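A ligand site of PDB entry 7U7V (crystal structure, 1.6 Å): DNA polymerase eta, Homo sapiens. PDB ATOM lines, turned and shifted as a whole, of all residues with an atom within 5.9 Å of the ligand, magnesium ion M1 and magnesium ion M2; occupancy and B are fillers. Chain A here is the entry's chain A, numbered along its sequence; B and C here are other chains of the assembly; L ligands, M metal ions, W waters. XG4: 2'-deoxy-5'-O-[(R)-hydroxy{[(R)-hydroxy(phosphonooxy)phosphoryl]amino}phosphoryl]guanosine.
Magnesium ion M1 is bound by the side-chain carboxylate of Asp 118 (2.1 Å), the side-chain carboxylate of Glu 119 (2.2 Å), water W4 (2.2 Å), water W7 (2.3 Å), the side-chain carboxylate of Asp 16 (2.3 Å) and an oxygen (O1A) of the ligand (2.3 Å).
O3' of DT 8 of chain B sits close to O2A of the ligand, 2.6 Å away. N1 of the ligand is in hydrogen-bond range of O2 of DT 4 of chain C, 2.6 Å away. OH of Tyr 55 sits at hydrogen-bond distance from O2G of the ligand (2.7 Å). O2G of the ligand lies within hydrogen-bond range of N of Cys 19. An oxygen (O3G) of the ligand is in salt-bridge range of the guanidinium group (NH2) of Arg 58 (3.1 Å). The backbone NH (N) of Phe 21 is in hydrogen-bond range of an oxygen (O3') of the ligand, at 3.0 Å. The guanidinium group of Arg 64 is in hydrogen-bond range of an oxygen (O6) of the ligand (3.1 Å). O2B of the ligand lies within hydrogen-bond range of N of Phe 20 (3.4 Å). O2G of the ligand lies within salt-bridge range of NZ of Lys 234. N2 of the ligand sits at hydrogen-bond distance from O4' of DA 5 of chain C, 3.3 Å away. N3 of DA 5 of chain C lies within hydrogen-bond range of a nitrogen (N1) of the ligand (3.4 Å).
Water W4 bridges O5' of the ligand (3.2 Å) and OG of Ser 116 (3.3 Å). Water W7 bridges NZ of Lys 227 (3.2 Å) and O2A of the ligand (3.3 Å). Water W1 lies within hydrogen-bond range of an oxygen (O2B) of the ligand (2.6 Å), the guanidinium group (NH2) of Arg 58 (2.9 Å) and the backbone NH (N) of Val 53 (2.9 Å). Water W6 lies within hydrogen-bond range of N2 of the ligand (2.7 Å) and N3 of DA 5 of chain C (3.3 Å). Water W3 lies within hydrogen-bond range of O of Ile 51 (3.0 Å) and N3A of the ligand (3.0 Å).
The backbone carbonyl oxygen of Asp 16 is in hydrogen-bond range of the side-chain amino group of Lys 234 (3.2 Å). N of Asp 118 sits at hydrogen-bond distance from OG of Ser 116 (3.0 Å). The side-chain hydroxyl (OG) of Ser 116 sits at hydrogen-bond distance from the backbone NH (N) of Glu 119, 3.1 Å away. The side-chain carboxylate (OE2) of Glu 119 is in salt-bridge range of the side-chain amino group (NZ) of Lys 227. O2 of DT 4 of chain C lies within hydrogen-bond range of the side-chain amide nitrogen (NE2) of Gln 41. O of Val 53 sits at hydrogen-bond distance from NE of Arg 58. O4 of DT 3 of chain C sits at hydrogen-bond distance from the guanidinium group of Arg 64 (2.7 Å). OD1 of Asp 18 is in salt-bridge range of NZ of Lys 234, 2.8 Å away.
Residues that only touch magnesium ion M2: Lys 234 (3.9 Å). Within 4 Å of magnesium ion M2: Asp 16, Met 17, Asp 118 and Lys 234.
OG of Ser 116 touches magnesium ion M1 (3.8 Å). Of the 25 residues printed, 4 come within 4 Å of magnesium ion M1.
Magnesium ion M2 is bound by the side-chain carboxylate (OD2) of Asp 16, 2.0 Å away. The side-chain carboxylate (OD2) of Asp 118 binds magnesium ion M2 (2.0 Å). Magnesium ion M2 is bound by O of Met 17. Magnesium ion M2 is bound by an oxygen (O1G) of the ligand (2.1 Å). An oxygen (O1B) of the ligand binds magnesium ion M2, 2.3 Å away. Magnesium ion M2 is bound by O1A of the ligand (2.3 Å). Magnesium ion M2 has six donor atoms within binding distance. Slightly farther from magnesium ion M2 lies the side-chain carboxylate (OD1) of Asp 16 (2.7 Å).
Asp 18 touches the ligand (CA to O2G, 3.2 Å). OE1 of Gln 41 touches N2 of the ligand, at 3.6 Å. Ile 51 touches the ligand. Ala 52 touches the ligand. Ile 117 touches the ligand (CG2 to O4', 3.9 Å). DT 3 of chain C touches the ligand (O4 to O6, 3.6 Å). Hydrophobic or aromatic side chains within 4 Å of the ligand: Phe 20, Phe 21, Ile 51, Ala 52, Tyr 55 and Ile 117. 19 residues have an atom within 4 Å of the ligand: Asp 16, Met 17, Asp 18, Cys 19, Phe 20, Phe 21, Gln 41, Ile 51, Ala 52, Tyr 55, Arg 58, Arg 64, Ile 117, Asp 118, Lys 234, DT 8 of chain B, DT 3 of chain C, DT 4 of chain C and DA 5 of chain C. The nearest printed residue that does not touch the ligand is Leu 92 (4.1 Å).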
ATOM      1  N   ASP A  16     -27.590 -24.745 -19.220  1.00  0.00           N
ATOM      2  CA  ASP A  16     -27.844 -24.584 -17.778  1.00  0.00           C
ATOM      3  C   ASP A  16     -28.029 -23.109 -17.426  1.00  0.00           C
ATOM      4  O   ASP A  16     -27.177 -22.301 -17.729  1.00  0.00           O
ATOM      5  CB  ASP A  16     -26.704 -25.124 -16.943  1.00  0.00           C
ATOM      6  CG  ASP A  16     -27.042 -24.861 -15.490  1.00  0.00           C
ATOM      7  OD1 ASP A  16     -27.749 -25.695 -14.924  1.00  0.00           O
ATOM      8  OD2 ASP A  16     -26.624 -23.845 -14.990  1.00  0.00           O
ATOM      9  N   MET A  17     -29.104 -22.846 -16.712  1.00  0.00           N
ATOM     10  CA  MET A  17     -29.393 -21.450 -16.325  1.00  0.00           C
ATOM     11  C   MET A  17     -28.365 -20.984 -15.282  1.00  0.00           C
ATOM     12  O   MET A  17     -28.067 -21.744 -14.393  1.00  0.00           O
ATOM     13  CB  MET A  17     -30.821 -21.332 -15.776  1.00  0.00           C
ATOM     14  CG  MET A  17     -31.880 -21.917 -16.671  1.00  0.00           C
ATOM     15  SD  MET A  17     -31.838 -21.261 -18.343  1.00  0.00           S
ATOM     16  CE  MET A  17     -32.146 -19.535 -18.034  1.00  0.00           C
ATOM     17  N   ASP A  18     -27.832 -19.788 -15.448  1.00  0.00           N
ATOM     18  CA  ASP A  18     -26.885 -19.220 -14.457  1.00  0.00           C
ATOM     19  C   ASP A  18     -27.655 -18.828 -13.180  1.00  0.00           C
ATOM     20  O   ASP A  18     -28.689 -18.218 -13.314  1.00  0.00           O
ATOM     21  CB  ASP A  18     -26.222 -17.960 -15.022  1.00  0.00           C
ATOM     22  CG  ASP A  18     -25.443 -18.187 -16.299  1.00  0.00           C
ATOM     23  OD1 ASP A  18     -24.922 -19.285 -16.478  1.00  0.00           O
ATOM     24  OD2 ASP A  18     -25.360 -17.259 -17.099  1.00  0.00           O
ATOM     25  N   CYS A  19     -27.116 -19.156 -12.003  1.00  0.00           N
ATOM     26  CA  CYS A  19     -27.728 -18.790 -10.685  1.00  0.00           C
ATOM     27  C   CYS A  19     -29.258 -18.701 -10.795  1.00  0.00           C
ATOM     28  O   CYS A  19     -29.789 -17.687 -10.450  1.00  0.00           O
ATOM     29  CB  CYS A  19     -27.015 -17.576 -10.107  1.00  0.00           C
ATOM     30  SG  CYS A  19     -26.890 -16.105 -11.147  1.00  0.00           S
ATOM     31  N   PHE A  20     -29.889 -19.808 -11.210  1.00  0.00           N
ATOM     32  CA  PHE A  20     -31.323 -19.743 -11.589  1.00  0.00           C
ATOM     33  C   PHE A  20     -32.243 -19.035 -10.586  1.00  0.00           C
ATOM     34  O   PHE A  20     -32.844 -18.046 -10.949  1.00  0.00           O
ATOM     35  CB  PHE A  20     -31.836 -21.123 -12.014  1.00  0.00           C
ATOM     36  CG  PHE A  20     -33.198 -21.105 -12.648  1.00  0.00           C
ATOM     37  CD1 PHE A  20     -33.492 -20.200 -13.666  1.00  0.00           C
ATOM     38  CD2 PHE A  20     -34.192 -21.970 -12.235  1.00  0.00           C
ATOM     39  CE1 PHE A  20     -34.745 -20.183 -14.248  1.00  0.00           C
ATOM     40  CE2 PHE A  20     -35.448 -21.940 -12.822  1.00  0.00           C
ATOM     41  CZ  PHE A  20     -35.712 -21.056 -13.830  1.00  0.00           C
ATOM     42  N   PHE A  21     -32.340 -19.586  -9.380  1.00  0.00           N
ATOM     43  CA  PHE A  21     -33.304 -19.004  -8.414  1.00  0.00           C
ATOM     44  C   PHE A  21     -32.988 -17.512  -8.202  1.00  0.00           C
ATOM     45  O   PHE A  21     -33.903 -16.735  -8.044  1.00  0.00           O
ATOM     46  CB  PHE A  21     -33.335 -19.815  -7.116  1.00  0.00           C
ATOM     47  CG  PHE A  21     -33.960 -21.186  -7.163  1.00  0.00           C
ATOM     48  CD1 PHE A  21     -34.090 -21.896  -8.345  1.00  0.00           C
ATOM     49  CD2 PHE A  21     -34.415 -21.786  -5.997  1.00  0.00           C
ATOM     50  CE1 PHE A  21     -34.644 -23.156  -8.367  1.00  0.00           C
ATOM     51  CE2 PHE A  21     -34.982 -23.042  -6.021  1.00  0.00           C
ATOM     52  CZ  PHE A  21     -35.100 -23.732  -7.198  1.00  0.00           C
ATOM     53  N   VAL A  22     -31.699 -17.178  -8.204  1.00  0.00           N
ATOM     54  CA  VAL A  22     -31.294 -15.752  -8.053  1.00  0.00           C
ATOM     55  C   VAL A  22     -31.832 -14.957  -9.247  1.00  0.00           C
ATOM     56  O   VAL A  22     -32.424 -13.918  -9.021  1.00  0.00           O
ATOM     57  CB  VAL A  22     -29.771 -15.600  -7.898  1.00  0.00           C
ATOM     58  CG1 VAL A  22     -29.299 -14.165  -8.055  1.00  0.00           C
ATOM     59  CG2 VAL A  22     -29.303 -16.155  -6.572  1.00  0.00           C
ATOM     60  N   GLN A  41     -33.510 -20.621   2.013  1.00  0.00           N
ATOM     61  CA  GLN A  41     -34.775 -21.147   2.511  1.00  0.00           C
ATOM     62  C   GLN A  41     -34.772 -21.161   4.034  1.00  0.00           C
ATOM     63  O   GLN A  41     -33.787 -21.535   4.669  1.00  0.00           O
ATOM     64  CB  GLN A  41     -35.136 -22.483   1.821  1.00  0.00           C
ATOM     65  CG  GLN A  41     -34.222 -23.628   1.908  1.00  0.00           C
ATOM     66  CD  GLN A  41     -34.471 -24.708   0.801  1.00  0.00           C
ATOM     67  OE1 GLN A  41     -35.387 -24.632  -0.056  1.00  0.00           O
ATOM     68  NE2 GLN A  41     -33.628 -25.682   0.811  1.00  0.00           N
ATOM     69  N   ILE A  51     -29.156 -21.582  -1.138  1.00  0.00           N
ATOM     70  CA  ILE A  51     -29.249 -22.568  -2.213  1.00  0.00           C
ATOM     71  C   ILE A  51     -28.886 -22.036  -3.596  1.00  0.00           C
ATOM     72  O   ILE A  51     -28.776 -22.841  -4.526  1.00  0.00           O
ATOM     73  CB  ILE A  51     -30.648 -23.243  -2.264  1.00  0.00           C
ATOM     74  CG1 ILE A  51     -31.744 -22.184  -2.426  1.00  0.00           C
ATOM     75  CG2 ILE A  51     -30.847 -24.221  -1.077  1.00  0.00           C
ATOM     76  CD1 ILE A  51     -33.099 -22.831  -2.707  1.00  0.00           C
ATOM     77  N   ALA A  52     -28.649 -20.727  -3.761  1.00  0.00           N
ATOM     78  CA  ALA A  52     -28.250 -20.164  -5.047  1.00  0.00           C
ATOM     79  C   ALA A  52     -27.563 -18.836  -4.793  1.00  0.00           C
ATOM     80  O   ALA A  52     -27.935 -18.132  -3.852  1.00  0.00           O
ATOM     81  CB  ALA A  52     -29.472 -19.953  -5.979  1.00  0.00           C
ATOM     82  N   VAL A  53     -26.551 -18.498  -5.623  1.00  0.00           N
ATOM     83  CA  VAL A  53     -25.623 -17.395  -5.364  1.00  0.00           C
ATOM     84  C   VAL A  53     -25.277 -16.684  -6.661  1.00  0.00           C
ATOM     85  O   VAL A  53     -24.779 -17.316  -7.607  1.00  0.00           O
ATOM     86  CB  VAL A  53     -24.329 -17.898  -4.698  1.00  0.00           C
ATOM     87  CG1 VAL A  53     -23.456 -16.727  -4.277  1.00  0.00           C
ATOM     88  CG2 VAL A  53     -24.614 -18.792  -3.525  1.00  0.00           C
ATOM     89  N   TYR A  55     -23.088 -14.395  -9.240  1.00  0.00           N
ATOM     90  CA  TYR A  55     -21.640 -14.444  -9.472  1.00  0.00           C
ATOM     91  C   TYR A  55     -20.909 -13.309  -8.751  1.00  0.00           C
ATOM     92  O   TYR A  55     -19.773 -13.496  -8.275  1.00  0.00           O
ATOM     93  CB  TYR A  55     -21.401 -14.433 -10.982  1.00  0.00           C
ATOM     94  CG  TYR A  55     -21.645 -15.839 -11.524  1.00  0.00           C
ATOM     95  CD1 TYR A  55     -22.933 -16.278 -11.768  1.00  0.00           C
ATOM     96  CD2 TYR A  55     -20.607 -16.722 -11.745  1.00  0.00           C
ATOM     97  CE1 TYR A  55     -23.185 -17.576 -12.229  1.00  0.00           C
ATOM     98  CE2 TYR A  55     -20.824 -18.005 -12.208  1.00  0.00           C
ATOM     99  CZ  TYR A  55     -22.121 -18.441 -12.441  1.00  0.00           C
ATOM    100  OH  TYR A  55     -22.351 -19.720 -12.906  1.00  0.00           O
ATOM    101  N   ARG A  58     -20.448 -14.739  -5.382  1.00  0.00           N
ATOM    102  CA  ARG A  58     -19.451 -15.811  -5.390  1.00  0.00           C
ATOM    103  C   ARG A  58     -18.049 -15.246  -5.285  1.00  0.00           C
ATOM    104  O   ARG A  58     -17.175 -15.894  -4.709  1.00  0.00           O
ATOM    105  CB  ARG A  58     -19.567 -16.662  -6.661  1.00  0.00           C
ATOM    106  CG  ARG A  58     -20.931 -17.302  -6.840  1.00  0.00           C
ATOM    107  CD  ARG A  58     -20.973 -18.151  -8.106  1.00  0.00           C
ATOM    108  NE  ARG A  58     -22.301 -18.729  -8.305  1.00  0.00           N
ATOM    109  CZ  ARG A  58     -22.543 -19.718  -9.149  1.00  0.00           C
ATOM    110  NH1 ARG A  58     -21.573 -20.270  -9.866  1.00  0.00           N
ATOM    111  NH2 ARG A  58     -23.795 -20.169  -9.286  1.00  0.00           N
ATOM    112  N   ARG A  64     -23.329 -22.264  -2.150  1.00  0.00           N
ATOM    113  CA  ARG A  64     -24.547 -23.006  -1.751  1.00  0.00           C
ATOM    114  C   ARG A  64     -24.189 -23.818  -0.497  1.00  0.00           C
ATOM    115  O   ARG A  64     -22.987 -24.067  -0.313  1.00  0.00           O
ATOM    116  CB  ARG A  64     -25.017 -23.862  -2.930  1.00  0.00           C
ATOM    117  CG  ARG A  64     -24.604 -25.315  -2.907  1.00  0.00           C
ATOM    118  CD  ARG A  64     -25.288 -26.033  -4.051  1.00  0.00           C
ATOM    119  NE  ARG A  64     -26.265 -27.012  -3.581  1.00  0.00           N
ATOM    120  CZ  ARG A  64     -25.970 -28.181  -3.012  1.00  0.00           C
ATOM    121  NH1 ARG A  64     -24.711 -28.536  -2.815  1.00  0.00           N
ATOM    122  NH2 ARG A  64     -26.933 -28.977  -2.617  1.00  0.00           N
ATOM    123  N   LEU A  92     -41.595 -24.278  -3.782  1.00  0.00           N
ATOM    124  CA  LEU A  92     -40.736 -23.881  -4.907  1.00  0.00           C
ATOM    125  C   LEU A  92     -41.512 -23.600  -6.203  1.00  0.00           C
ATOM    126  O   LEU A  92     -40.908 -23.600  -7.283  1.00  0.00           O
ATOM    127  CB  LEU A  92     -39.678 -24.949  -5.154  1.00  0.00           C
ATOM    128  CG  LEU A  92     -38.860 -25.326  -3.905  1.00  0.00           C
ATOM    129  CD1 LEU A  92     -37.950 -26.520  -4.153  1.00  0.00           C
ATOM    130  CD2 LEU A  92     -38.082 -24.123  -3.411  1.00  0.00           C
ATOM    131  N   SER A 116     -32.878 -31.265 -14.968  1.00  0.00           N
ATOM    132  CA  SER A 116     -33.112 -30.664 -13.642  1.00  0.00           C
ATOM    133  C   SER A 116     -34.046 -29.470 -13.830  1.00  0.00           C
ATOM    134  O   SER A 116     -34.390 -29.192 -14.967  1.00  0.00           O
ATOM    135  CB  SER A 116     -31.834 -30.209 -13.003  1.00  0.00           C
ATOM    136  OG  SER A 116     -31.464 -28.922 -13.471  1.00  0.00           O
ATOM    137  N   ILE A 117     -34.375 -28.785 -12.748  1.00  0.00           N
ATOM    138  CA  ILE A 117     -35.215 -27.559 -12.829  1.00  0.00           C
ATOM    139  C   ILE A 117     -34.562 -26.508 -13.736  1.00  0.00           C
ATOM    140  O   ILE A 117     -35.275 -25.695 -14.282  1.00  0.00           O
ATOM    141  CB  ILE A 117     -35.456 -26.999 -11.407  1.00  0.00           C
ATOM    142  CG1 ILE A 117     -36.678 -26.081 -11.346  1.00  0.00           C
ATOM    143  CG2 ILE A 117     -34.217 -26.328 -10.829  1.00  0.00           C
ATOM    144  CD1 ILE A 117     -37.183 -25.842  -9.958  1.00  0.00           C
ATOM    145  N   ASP A 118     -33.244 -26.552 -13.901  1.00  0.00           N
ATOM    146  CA  ASP A 118     -32.610 -25.431 -14.644  1.00  0.00           C
ATOM    147  C   ASP A 118     -31.735 -25.921 -15.795  1.00  0.00           C
ATOM    148  O   ASP A 118     -31.073 -25.092 -16.406  1.00  0.00           O
ATOM    149  CB  ASP A 118     -31.852 -24.541 -13.673  1.00  0.00           C
ATOM    150  CG  ASP A 118     -30.403 -24.907 -13.512  1.00  0.00           C
ATOM    151  OD1 ASP A 118     -30.114 -26.095 -13.260  1.00  0.00           O
ATOM    152  OD2 ASP A 118     -29.577 -23.992 -13.629  1.00  0.00           O
ATOM    153  N   GLU A 119     -31.750 -27.220 -16.082  1.00  0.00           N
ATOM    154  CA  GLU A 119     -30.901 -27.613 -17.228  1.00  0.00           C
ATOM    155  C   GLU A 119     -31.575 -28.654 -18.117  1.00  0.00           C
ATOM    156  O   GLU A 119     -32.387 -29.434 -17.629  1.00  0.00           O
ATOM    157  CB  GLU A 119     -29.545 -28.154 -16.791  1.00  0.00           C
ATOM    158  CG  GLU A 119     -29.544 -29.570 -16.307  1.00  0.00           C
ATOM    159  CD  GLU A 119     -28.451 -29.643 -15.270  1.00  0.00           C
ATOM    160  OE1 GLU A 119     -28.583 -28.905 -14.280  1.00  0.00           O
ATOM    161  OE2 GLU A 119     -27.457 -30.345 -15.500  1.00  0.00           O
ATOM    162  N   LYS A 227     -22.041 -31.458 -20.853  1.00  0.00           N
ATOM    163  CA  LYS A 227     -22.176 -31.000 -19.471  1.00  0.00           C
ATOM    164  C   LYS A 227     -20.859 -30.416 -18.958  1.00  0.00           C
ATOM    165  O   LYS A 227     -20.830 -29.340 -18.362  1.00  0.00           O
ATOM    166  CB  LYS A 227     -22.625 -32.162 -18.586  1.00  0.00           C
ATOM    167  CG  LYS A 227     -22.679 -31.877 -17.063  1.00  0.00           C
ATOM    168  CD  LYS A 227     -23.652 -30.756 -16.749  1.00  0.00           C
ATOM    169  CE  LYS A 227     -23.856 -30.610 -15.235  1.00  0.00           C
ATOM    170  NZ  LYS A 227     -24.820 -29.509 -14.918  1.00  0.00           N
ATOM    171  N   LYS A 234     -18.535 -20.153 -17.491  1.00  0.00           N
ATOM    172  CA  LYS A 234     -19.746 -19.599 -16.924  1.00  0.00           C
ATOM    173  C   LYS A 234     -19.370 -18.273 -16.285  1.00  0.00           C
ATOM    174  O   LYS A 234     -18.244 -18.133 -15.785  1.00  0.00           O
ATOM    175  CB  LYS A 234     -20.343 -20.541 -15.874  1.00  0.00           C
ATOM    176  CG  LYS A 234     -21.380 -21.558 -16.380  1.00  0.00           C
ATOM    177  CD  LYS A 234     -22.284 -22.109 -15.249  1.00  0.00           C
ATOM    178  CE  LYS A 234     -23.607 -22.721 -15.770  1.00  0.00           C
ATOM    179  NZ  LYS A 234     -24.839 -21.886 -15.541  1.00  0.00           N
ATOM    180  P    DT B   8     -23.930 -31.540 -10.041  1.00  0.00           P
ATOM    181  OP1  DT B   8     -23.695 -31.163 -11.449  1.00  0.00           O
ATOM    182  OP2  DT B   8     -22.793 -31.744  -9.124  1.00  0.00           O
ATOM    183  O5'  DT B   8     -24.875 -30.425  -9.406  1.00  0.00           O
ATOM    184  C5'  DT B   8     -26.314 -30.500  -9.491  1.00  0.00           C
ATOM    185  C4'  DT B   8     -26.908 -29.693  -8.364  1.00  0.00           C
ATOM    186  O4'  DT B   8     -27.461 -30.552  -7.343  1.00  0.00           O
ATOM    187  C3'  DT B   8     -25.891 -28.770  -7.651  1.00  0.00           C
ATOM    188  O3'  DT B   8     -26.253 -27.407  -7.326  1.00  0.00           O
ATOM    189  C2'  DT B   8     -25.713 -29.448  -6.313  1.00  0.00           C
ATOM    190  C1'  DT B   8     -27.112 -29.963  -6.121  1.00  0.00           C
ATOM    191  N1   DT B   8     -27.240 -30.966  -5.073  1.00  0.00           N
ATOM    192  C2   DT B   8     -28.484 -31.169  -4.555  1.00  0.00           C
ATOM    193  O2   DT B   8     -29.482 -30.595  -4.976  1.00  0.00           O
ATOM    194  N3   DT B   8     -28.542 -32.070  -3.528  1.00  0.00           N
ATOM    195  C4   DT B   8     -27.484 -32.776  -2.984  1.00  0.00           C
ATOM    196  O4   DT B   8     -27.685 -33.564  -2.061  1.00  0.00           O
ATOM    197  C5   DT B   8     -26.191 -32.496  -3.571  1.00  0.00           C
ATOM    198  C7   DT B   8     -24.990 -33.205  -3.039  1.00  0.00           C
ATOM    199  C6   DT B   8     -26.137 -31.611  -4.561  1.00  0.00           C
ATOM    200  P    DT C   3     -25.463 -29.030   9.681  1.00  0.00           P
ATOM    201  OP1  DT C   3     -24.767 -30.198  10.299  1.00  0.00           O
ATOM    202  OP2  DT C   3     -24.695 -27.820   9.360  1.00  0.00           O
ATOM    203  O5'  DT C   3     -26.111 -29.485   8.298  1.00  0.00           O
ATOM    204  C5'  DT C   3     -26.076 -28.594   7.180  1.00  0.00           C
ATOM    205  C4'  DT C   3     -27.455 -28.036   6.933  1.00  0.00           C
ATOM    206  O4'  DT C   3     -27.488 -27.351   5.666  1.00  0.00           O
ATOM    207  C3'  DT C   3     -28.540 -29.103   6.852  1.00  0.00           C
ATOM    208  O3'  DT C   3     -29.794 -28.692   7.434  1.00  0.00           O
ATOM    209  C2'  DT C   3     -28.695 -29.311   5.365  1.00  0.00           C
ATOM    210  C1'  DT C   3     -28.530 -27.894   4.868  1.00  0.00           C
ATOM    211  N1   DT C   3     -28.145 -27.800   3.506  1.00  0.00           N
ATOM    212  C2   DT C   3     -28.778 -26.922   2.669  1.00  0.00           C
ATOM    213  O2   DT C   3     -29.680 -26.182   3.022  1.00  0.00           O
ATOM    214  N3   DT C   3     -28.324 -26.932   1.376  1.00  0.00           N
ATOM    215  C4   DT C   3     -27.339 -27.748   0.866  1.00  0.00           C
ATOM    216  O4   DT C   3     -27.000 -27.631  -0.298  1.00  0.00           O
ATOM    217  C5   DT C   3     -26.704 -28.633   1.799  1.00  0.00           C
ATOM    218  C7   DT C   3     -25.610 -29.528   1.340  1.00  0.00           C
ATOM    219  C6   DT C   3     -27.133 -28.606   3.062  1.00  0.00           C
ATOM    220  P    DT C   4     -31.087 -29.618   7.394  1.00  0.00           P
ATOM    221  OP1  DT C   4     -31.954 -29.203   8.512  1.00  0.00           O
ATOM    222  OP2  DT C   4     -30.646 -31.030   7.292  1.00  0.00           O
ATOM    223  O5'  DT C   4     -31.868 -29.143   6.099  1.00  0.00           O
ATOM    224  C5'  DT C   4     -32.154 -27.759   5.889  1.00  0.00           C
ATOM    225  C4'  DT C   4     -33.074 -27.600   4.697  1.00  0.00           C
ATOM    226  O4'  DT C   4     -32.316 -27.654   3.476  1.00  0.00           O
ATOM    227  C3'  DT C   4     -34.145 -28.677   4.565  1.00  0.00           C
ATOM    228  O3'  DT C   4     -35.266 -28.008   4.023  1.00  0.00           O
ATOM    229  C2'  DT C   4     -33.573 -29.629   3.535  1.00  0.00           C
ATOM    230  C1'  DT C   4     -32.800 -28.683   2.628  1.00  0.00           C
ATOM    231  N1   DT C   4     -31.638 -29.271   1.946  1.00  0.00           N
ATOM    232  C2   DT C   4     -31.421 -28.884   0.651  1.00  0.00           C
ATOM    233  O2   DT C   4     -32.132 -28.084   0.073  1.00  0.00           O
ATOM    234  N3   DT C   4     -30.310 -29.423   0.082  1.00  0.00           N
ATOM    235  C4   DT C   4     -29.426 -30.308   0.644  1.00  0.00           C
ATOM    236  O4   DT C   4     -28.481 -30.721  -0.004  1.00  0.00           O
ATOM    237  C5   DT C   4     -29.710 -30.671   2.018  1.00  0.00           C
ATOM    238  C7   DT C   4     -28.826 -31.665   2.696  1.00  0.00           C
ATOM    239  C6   DT C   4     -30.802 -30.143   2.586  1.00  0.00           C
ATOM    240  P    DA C   5     -36.587 -28.869   3.715  1.00  0.00           P
ATOM    241  OP1  DA C   5     -37.753 -28.031   4.072  1.00  0.00           O
ATOM    242  OP2  DA C   5     -36.423 -30.223   4.263  1.00  0.00           O
ATOM    243  O5'  DA C   5     -36.575 -29.003   2.125  1.00  0.00           O
ATOM    244  C5'  DA C   5     -36.662 -27.836   1.320  1.00  0.00           C
ATOM    245  C4'  DA C   5     -36.812 -28.213  -0.128  1.00  0.00           C
ATOM    246  O4'  DA C   5     -35.563 -28.792  -0.621  1.00  0.00           O
ATOM    247  C3'  DA C   5     -37.885 -29.252  -0.398  1.00  0.00           C
ATOM    248  O3'  DA C   5     -38.520 -28.963  -1.636  1.00  0.00           O
ATOM    249  C2'  DA C   5     -37.098 -30.564  -0.443  1.00  0.00           C
ATOM    250  C1'  DA C   5     -35.769 -30.120  -1.047  1.00  0.00           C
ATOM    251  N9   DA C   5     -34.605 -30.913  -0.647  1.00  0.00           N
ATOM    252  C8   DA C   5     -34.410 -31.541   0.555  1.00  0.00           C
ATOM    253  N7   DA C   5     -33.252 -32.161   0.654  1.00  0.00           N
ATOM    254  C5   DA C   5     -32.638 -31.904  -0.567  1.00  0.00           C
ATOM    255  C6   DA C   5     -31.391 -32.284  -1.105  1.00  0.00           C
ATOM    256  N6   DA C   5     -30.497 -33.041  -0.443  1.00  0.00           N
ATOM    257  N1   DA C   5     -31.093 -31.866  -2.350  1.00  0.00           N
ATOM    258  C2   DA C   5     -31.987 -31.110  -3.012  1.00  0.00           C
ATOM    259  N3   DA C   5     -33.192 -30.698  -2.613  1.00  0.00           N
ATOM    260  C4   DA C   5     -33.458 -31.131  -1.366  1.00  0.00           C
HETATM  261  N1  XG4 L   1     -32.012 -27.541  -2.510  1.00  0.00           N
HETATM  262  C2  XG4 L   1     -32.930 -26.848  -3.262  1.00  0.00           C
HETATM  263  N2  XG4 L   1     -34.159 -26.761  -2.747  1.00  0.00           N
HETATM  264  N3  XG4 L   1     -32.692 -26.253  -4.437  1.00  0.00           N
HETATM  265  C4  XG4 L   1     -31.439 -26.371  -4.851  1.00  0.00           C
HETATM  266  C5  XG4 L   1     -30.438 -27.026  -4.206  1.00  0.00           C
HETATM  267  C6  XG4 L   1     -30.752 -27.637  -2.970  1.00  0.00           C
HETATM  268  O6  XG4 L   1     -29.917 -28.257  -2.302  1.00  0.00           O
HETATM  269  N7  XG4 L   1     -29.252 -26.924  -4.926  1.00  0.00           N
HETATM  270  C8  XG4 L   1     -29.569 -26.199  -5.971  1.00  0.00           C
HETATM  271  N9  XG4 L   1     -30.888 -25.829  -5.981  1.00  0.00           N
HETATM  272  PA  XG4 L   1     -27.633 -25.286 -10.281  1.00  0.00           P
HETATM  273  PB  XG4 L   1     -27.279 -22.387 -10.306  1.00  0.00           P
HETATM  274  PG  XG4 L   1     -24.931 -22.133 -11.898  1.00  0.00           P
HETATM  275  C1' XG4 L   1     -31.607 -24.944  -6.908  1.00  0.00           C
HETATM  276  O1A XG4 L   1     -27.629 -25.288 -11.749  1.00  0.00           O
HETATM  277  O1B XG4 L   1     -28.230 -22.424 -11.426  1.00  0.00           O
HETATM  278  O1G XG4 L   1     -25.580 -23.194 -12.715  1.00  0.00           O
HETATM  279  C2' XG4 L   1     -31.159 -23.487  -6.858  1.00  0.00           C
HETATM  280  O2A XG4 L   1     -26.710 -26.422  -9.670  1.00  0.00           O
HETATM  281  O2B XG4 L   1     -27.790 -21.478  -9.144  1.00  0.00           O
HETATM  282  O2G XG4 L   1     -24.796 -20.812 -12.620  1.00  0.00           O
HETATM  283  C3' XG4 L   1     -30.391 -23.291  -8.161  1.00  0.00           C
HETATM  284  O3' XG4 L   1     -30.573 -21.945  -8.621  1.00  0.00           O
HETATM  285  N3A XG4 L   1     -27.071 -23.880  -9.683  1.00  0.00           N
HETATM  286  O3B XG4 L   1     -25.846 -21.819 -10.639  1.00  0.00           O
HETATM  287  O3G XG4 L   1     -23.579 -22.544 -11.288  1.00  0.00           O
HETATM  288  C4' XG4 L   1     -31.044 -24.314  -9.093  1.00  0.00           C
HETATM  289  O4' XG4 L   1     -31.394 -25.413  -8.242  1.00  0.00           O
HETATM  290  C5' XG4 L   1     -30.188 -24.810 -10.230  1.00  0.00           C
HETATM  291  O5' XG4 L   1     -29.076 -25.554  -9.679  1.00  0.00           O
HETATM  292 MG    MG M   1     -28.217 -27.073 -13.147  1.00  0.00          MG
HETATM  293 MG    MG M   2     -27.620 -23.532 -13.298  1.00  0.00          MG
HETATM  294  O   HOH W   1     -25.959 -20.639  -7.480  1.00  0.00           O
HETATM  295  O   HOH W   2     -24.293 -25.485 -12.843  1.00  0.00           O
HETATM  296  O   HOH W   3     -26.932 -23.788  -6.684  1.00  0.00           O
HETATM  297  O   HOH W   4     -29.029 -28.251 -11.417  1.00  0.00           O
HETATM  298  O   HOH W   5     -23.098 -23.619  -8.969  1.00  0.00           O
HETATM  299  O   HOH W   6     -34.984 -28.709  -4.479  1.00  0.00           O
HETATM  300  O   HOH W   7     -26.077 -27.643 -12.637  1.00  0.00           O
HETATM  301  O   HOH W   8     -31.229 -28.159  -8.650  1.00  0.00           O
